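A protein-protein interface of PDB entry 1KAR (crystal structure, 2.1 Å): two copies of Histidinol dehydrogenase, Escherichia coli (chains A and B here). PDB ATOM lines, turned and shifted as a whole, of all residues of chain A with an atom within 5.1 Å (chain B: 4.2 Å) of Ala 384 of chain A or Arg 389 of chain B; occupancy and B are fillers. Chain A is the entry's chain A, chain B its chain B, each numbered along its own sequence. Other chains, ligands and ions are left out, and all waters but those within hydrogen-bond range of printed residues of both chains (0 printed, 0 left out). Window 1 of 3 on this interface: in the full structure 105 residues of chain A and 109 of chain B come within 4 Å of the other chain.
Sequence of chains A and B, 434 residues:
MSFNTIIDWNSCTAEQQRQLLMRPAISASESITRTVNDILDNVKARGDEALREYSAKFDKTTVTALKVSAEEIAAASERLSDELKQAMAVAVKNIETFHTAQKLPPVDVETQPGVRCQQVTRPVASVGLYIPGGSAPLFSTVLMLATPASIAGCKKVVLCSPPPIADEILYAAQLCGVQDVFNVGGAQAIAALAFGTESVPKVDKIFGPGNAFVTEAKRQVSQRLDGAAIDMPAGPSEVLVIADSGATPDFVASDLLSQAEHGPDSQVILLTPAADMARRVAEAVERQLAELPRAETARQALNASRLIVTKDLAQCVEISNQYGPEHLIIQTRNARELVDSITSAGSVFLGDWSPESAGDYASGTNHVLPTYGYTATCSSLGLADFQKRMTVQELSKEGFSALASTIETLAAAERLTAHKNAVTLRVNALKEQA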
ATOM      1  N   GLN A 102     -11.492   4.818 -10.555  1.00  0.00           N
ATOM      2  CA  GLN A 102     -10.610   5.831  -9.983  1.00  0.00           C
ATOM      3  C   GLN A 102     -10.361   7.044 -10.892  1.00  0.00           C
ATOM      4  O   GLN A 102      -9.685   7.992 -10.497  1.00  0.00           O
ATOM      5  CB  GLN A 102      -9.269   5.191  -9.615  1.00  0.00           C
ATOM      6  CG  GLN A 102      -9.367   4.137  -8.529  1.00  0.00           C
ATOM      7  CD  GLN A 102      -8.090   3.337  -8.379  1.00  0.00           C
ATOM      8  OE1 GLN A 102      -6.998   3.871  -8.521  1.00  0.00           O
ATOM      9  NE2 GLN A 102      -8.225   2.050  -8.077  1.00  0.00           N
ATOM     10  N   GLY A 346      -2.038   0.746   4.096  1.00  0.00           N
ATOM     11  CA  GLY A 346      -1.967   0.633   2.649  1.00  0.00           C
ATOM     12  C   GLY A 346      -3.299   0.158   2.092  1.00  0.00           C
ATOM     13  O   GLY A 346      -3.950   0.832   1.288  1.00  0.00           O
ATOM     14  N   CYS A 378       2.803   7.999   1.029  1.00  0.00           N
ATOM     15  CA  CYS A 378       2.620   7.317  -0.247  1.00  0.00           C
ATOM     16  C   CYS A 378       1.304   6.534  -0.268  1.00  0.00           C
ATOM     17  O   CYS A 378       0.720   6.240   0.784  1.00  0.00           O
ATOM     18  CB  CYS A 378       3.815   6.394  -0.521  1.00  0.00           C
ATOM     19  SG  CYS A 378       3.794   5.608  -2.172  1.00  0.00           S
ATOM     20  N   SER A 379       0.837   6.190  -1.461  1.00  0.00           N
ATOM     21  CA  SER A 379      -0.420   5.470  -1.579  1.00  0.00           C
ATOM     22  C   SER A 379      -0.320   4.171  -2.351  1.00  0.00           C
ATOM     23  O   SER A 379       0.672   3.902  -3.022  1.00  0.00           O
ATOM     24  CB  SER A 379      -1.456   6.362  -2.256  1.00  0.00           C
ATOM     25  OG  SER A 379      -1.572   7.593  -1.569  1.00  0.00           O
ATOM     26  N   SER A 380      -1.360   3.355  -2.244  1.00  0.00           N
ATOM     27  CA  SER A 380      -1.404   2.114  -2.988  1.00  0.00           C
ATOM     28  C   SER A 380      -1.297   2.467  -4.460  1.00  0.00           C
ATOM     29  O   SER A 380      -1.663   3.571  -4.872  1.00  0.00           O
ATOM     30  CB  SER A 380      -2.731   1.395  -2.778  1.00  0.00           C
ATOM     31  OG  SER A 380      -2.930   0.440  -3.811  1.00  0.00           O
ATOM     32  N   LEU A 381      -0.791   1.530  -5.251  1.00  0.00           N
ATOM     33  CA  LEU A 381      -0.685   1.753  -6.678  1.00  0.00           C
ATOM     34  C   LEU A 381      -2.126   1.828  -7.177  1.00  0.00           C
ATOM     35  O   LEU A 381      -2.982   1.043  -6.750  1.00  0.00           O
ATOM     36  CB  LEU A 381       0.031   0.581  -7.348  1.00  0.00           C
ATOM     37  CG  LEU A 381       0.443   0.760  -8.808  1.00  0.00           C
ATOM     38  CD1 LEU A 381       1.514   1.809  -8.896  1.00  0.00           C
ATOM     39  CD2 LEU A 381       0.956  -0.555  -9.365  1.00  0.00           C
ATOM     40  N   GLY A 382      -2.386   2.783  -8.061  1.00  0.00           N
ATOM     41  CA  GLY A 382      -3.719   2.952  -8.613  1.00  0.00           C
ATOM     42  C   GLY A 382      -3.597   3.613  -9.968  1.00  0.00           C
ATOM     43  O   GLY A 382      -2.499   3.732 -10.495  1.00  0.00           O
ATOM     44  N   LEU A 383      -4.713   4.052 -10.532  1.00  0.00           N
ATOM     45  CA  LEU A 383      -4.698   4.690 -11.842  1.00  0.00           C
ATOM     46  C   LEU A 383      -3.754   5.887 -11.867  1.00  0.00           C
ATOM     47  O   LEU A 383      -2.995   6.091 -12.821  1.00  0.00           O
ATOM     48  CB  LEU A 383      -6.108   5.162 -12.201  1.00  0.00           C
ATOM     49  CG  LEU A 383      -6.319   5.724 -13.606  1.00  0.00           C
ATOM     50  CD1 LEU A 383      -5.997   4.648 -14.649  1.00  0.00           C
ATOM     51  CD2 LEU A 383      -7.767   6.193 -13.743  1.00  0.00           C
ATOM     52  N   ALA A 384      -3.812   6.672 -10.800  1.00  0.00           N
ATOM     53  CA  ALA A 384      -3.013   7.879 -10.669  1.00  0.00           C
ATOM     54  C   ALA A 384      -1.507   7.712 -10.894  1.00  0.00           C
ATOM     55  O   ALA A 384      -0.836   8.651 -11.302  1.00  0.00           O
ATOM     56  CB  ALA A 384      -3.273   8.502  -9.308  1.00  0.00           C
ATOM     57  N   ASP A 385      -0.971   6.524 -10.637  1.00  0.00           N
ATOM     58  CA  ASP A 385       0.463   6.298 -10.805  1.00  0.00           C
ATOM     59  C   ASP A 385       0.897   6.128 -12.272  1.00  0.00           C
ATOM     60  O   ASP A 385       2.091   6.067 -12.558  1.00  0.00           O
ATOM     61  CB  ASP A 385       0.896   5.070  -9.989  1.00  0.00           C
ATOM     62  CG  ASP A 385       0.732   5.270  -8.489  1.00  0.00           C
ATOM     63  OD1 ASP A 385       1.602   5.924  -7.874  1.00  0.00           O
ATOM     64  OD2 ASP A 385      -0.273   4.777  -7.922  1.00  0.00           O
ATOM     65  N   PHE A 386      -0.066   6.048 -13.191  1.00  0.00           N
ATOM     66  CA  PHE A 386       0.246   5.891 -14.613  1.00  0.00           C
ATOM     67  C   PHE A 386      -0.214   7.081 -15.431  1.00  0.00           C
ATOM     68  O   PHE A 386      -0.415   6.963 -16.641  1.00  0.00           O
ATOM     69  CB  PHE A 386      -0.412   4.643 -15.205  1.00  0.00           C
ATOM     70  CG  PHE A 386       0.000   3.370 -14.547  1.00  0.00           C
ATOM     71  CD1 PHE A 386      -0.540   2.997 -13.318  1.00  0.00           C
ATOM     72  CD2 PHE A 386       0.940   2.539 -15.151  1.00  0.00           C
ATOM     73  CE1 PHE A 386      -0.146   1.806 -12.697  1.00  0.00           C
ATOM     74  CE2 PHE A 386       1.339   1.355 -14.539  1.00  0.00           C
ATOM     75  CZ  PHE A 386       0.793   0.991 -13.312  1.00  0.00           C
ATOM     76  N   GLN A 387      -0.383   8.220 -14.771  1.00  0.00           N
ATOM     77  CA  GLN A 387      -0.816   9.424 -15.449  1.00  0.00           C
ATOM     78  C   GLN A 387      -0.354  10.628 -14.644  1.00  0.00           C
ATOM     79  O   GLN A 387       0.327  10.477 -13.633  1.00  0.00           O
ATOM     80  CB  GLN A 387      -2.340   9.415 -15.605  1.00  0.00           C
ATOM     81  CG  GLN A 387      -3.122   9.431 -14.303  1.00  0.00           C
ATOM     82  CD  GLN A 387      -4.618   9.255 -14.517  1.00  0.00           C
ATOM     83  OE1 GLN A 387      -5.425   9.579 -13.645  1.00  0.00           O
ATOM     84  NE2 GLN A 387      -4.992   8.730 -15.675  1.00  0.00           N
ATOM     85  N   LYS A 388      -0.692  11.826 -15.105  1.00  0.00           N
ATOM     86  CA  LYS A 388      -0.298  13.031 -14.386  1.00  0.00           C
ATOM     87  C   LYS A 388      -1.348  14.111 -14.589  1.00  0.00           C
ATOM     88  O   LYS A 388      -2.033  14.130 -15.614  1.00  0.00           O
ATOM     89  CB  LYS A 388       1.078  13.531 -14.858  1.00  0.00           C
ATOM     90  CG  LYS A 388       1.080  14.266 -16.195  1.00  0.00           C
ATOM     91  CD  LYS A 388       0.933  13.313 -17.372  1.00  0.00           C
ATOM     92  CE  LYS A 388       2.271  13.005 -18.028  1.00  0.00           C
ATOM     93  NZ  LYS A 388       2.843  14.185 -18.743  1.00  0.00           N
ATOM     94  N   GLN B 119     -11.835   3.407  -2.341  1.00  0.00           N
ATOM     95  CA  GLN B 119     -10.600   4.167  -2.336  1.00  0.00           C
ATOM     96  C   GLN B 119     -10.953   5.396  -1.516  1.00  0.00           C
ATOM     97  O   GLN B 119     -11.802   6.184  -1.918  1.00  0.00           O
ATOM     98  CB  GLN B 119     -10.222   4.614  -3.744  1.00  0.00           C
ATOM     99  CG  GLN B 119      -8.928   5.396  -3.803  1.00  0.00           C
ATOM    100  CD  GLN B 119      -8.705   6.027  -5.160  1.00  0.00           C
ATOM    101  OE1 GLN B 119      -9.308   7.057  -5.486  1.00  0.00           O
ATOM    102  NE2 GLN B 119      -7.848   5.412  -5.966  1.00  0.00           N
ATOM    103  N   VAL B 120     -10.340   5.553  -0.353  1.00  0.00           N
ATOM    104  CA  VAL B 120     -10.630   6.726   0.458  1.00  0.00           C
ATOM    105  C   VAL B 120      -9.348   7.533   0.630  1.00  0.00           C
ATOM    106  O   VAL B 120      -8.241   6.988   0.560  1.00  0.00           O
ATOM    107  CB  VAL B 120     -11.210   6.339   1.845  1.00  0.00           C
ATOM    108  CG1 VAL B 120     -12.491   5.536   1.658  1.00  0.00           C
ATOM    109  CG2 VAL B 120     -10.195   5.555   2.647  1.00  0.00           C
ATOM    110  N   LYS B 388      -3.299  11.111   0.871  1.00  0.00           N
ATOM    111  CA  LYS B 388      -2.932   9.720   0.601  1.00  0.00           C
ATOM    112  C   LYS B 388      -4.191   8.944   0.226  1.00  0.00           C
ATOM    113  O   LYS B 388      -5.262   9.171   0.799  1.00  0.00           O
ATOM    114  CB  LYS B 388      -2.344   9.055   1.846  1.00  0.00           C
ATOM    115  CG  LYS B 388      -1.252   9.827   2.539  1.00  0.00           C
ATOM    116  CD  LYS B 388      -0.882   9.145   3.834  1.00  0.00           C
ATOM    117  CE  LYS B 388      -2.089   9.015   4.750  1.00  0.00           C
ATOM    118  NZ  LYS B 388      -1.735   8.275   5.983  1.00  0.00           N
ATOM    119  N   ARG B 389      -4.055   8.029  -0.724  1.00  0.00           N
ATOM    120  CA  ARG B 389      -5.162   7.190  -1.158  1.00  0.00           C
ATOM    121  C   ARG B 389      -5.012   5.862  -0.434  1.00  0.00           C
ATOM    122  O   ARG B 389      -3.950   5.243  -0.455  1.00  0.00           O
ATOM    123  CB  ARG B 389      -5.127   6.964  -2.677  1.00  0.00           C
ATOM    124  CG  ARG B 389      -5.668   8.142  -3.495  1.00  0.00           C
ATOM    125  CD  ARG B 389      -5.557   7.906  -5.002  1.00  0.00           C
ATOM    126  NE  ARG B 389      -4.171   7.810  -5.466  1.00  0.00           N
ATOM    127  CZ  ARG B 389      -3.566   6.671  -5.810  1.00  0.00           C
ATOM    128  NH1 ARG B 389      -4.224   5.523  -5.746  1.00  0.00           N
ATOM    129  NH2 ARG B 389      -2.303   6.679  -6.223  1.00  0.00           N
ATOM    130  N   MET B 390      -6.082   5.444   0.219  1.00  0.00           N
ATOM    131  CA  MET B 390      -6.098   4.210   0.972  1.00  0.00           C
ATOM    132  C   MET B 390      -7.188   3.303   0.390  1.00  0.00           C
ATOM    133  O   MET B 390      -8.301   3.750   0.084  1.00  0.00           O
ATOM    134  CB  MET B 390      -6.364   4.543   2.444  1.00  0.00           C
ATOM    135  CG  MET B 390      -6.420   3.359   3.383  1.00  0.00           C
ATOM    136  SD  MET B 390      -6.270   3.908   5.233  1.00  0.00           S
ATOM    137  CE  MET B 390      -8.093   4.489   5.558  1.00  0.00           C
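The side-chain amide oxygen (OE1) of Gln 102 of chain A is in hydrogen-bond range of the side-chain amide nitrogen (NE2) of Gln 119 of chain B, at 3.1 Å.
OG of Ser 379 of chain A lies within hydrogen-bond range of N of Arg 389 of chain B, 2.7 Å away.
The backbone carbonyl oxygen of Ser 380 of chain A lies within hydrogen-bond range of the guanidinium group of Arg 389 of chain B (3.3 Å).
The side-chain carboxylate (OD2) of Asp 385 of chain A lies within salt-bridge range of the guanidinium group (NH2) of Arg 389 of chain B (3.3 Å).
Hydrophobic or aromatic side chains of chain A that line the printed part of chain B: Ala 384.
Among the printed residues, 7 pairs touch across the chains.
Among the printed residues, pairs that only touch across the chains: Ser 379 of chain A with Lys 388 of chain B, Gly 382 of chain A with Arg 389 of chain B and Ala 384 of chain A with Arg 389 of chain B.
Of chain B, only Arg 389 (3.7 Å) comes within 4 Å of Ala 384 of chain A.
Of chain A, only Ser 379 (2.7 Å), Ser 380 (3.3 Å), Gly 382 (3.9 Å), Ala 384 (3.7 Å) and Asp 385 (3.3 Å) come within 4 Å of Arg 389 of chain B.
Of the printed residues of chain B, Ser 380 of chain A touches Arg 389.
Of the printed residues of chain B, Asp 385 of chain A touches Arg 389 (3.3 Å).
Gly 346 of chain A touches none of the printed residues of chain B.
The nearest printed residue of chain B that does not touch Ala 384 of chain A is Gln 119 of chain B (6.4 Å).
The nearest residue of chain A that does not touch Arg 389 of chain B is Gln 102 of chain A (4.3 Å).
The nearest printed residue of chain B that does not touch Asp 385 of chain A is Gln 119 of chain B (7.8 Å).
Position printed for both chains: 388.
OE1 of Gln 102 of chain A is in hydrogen-bond range of N of Leu 383 of chain A, 3.0 Å away.
The backbone NH of Gly 382 of chain A sits at hydrogen-bond distance from the side-chain carboxylate of Asp 385 of chain A.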
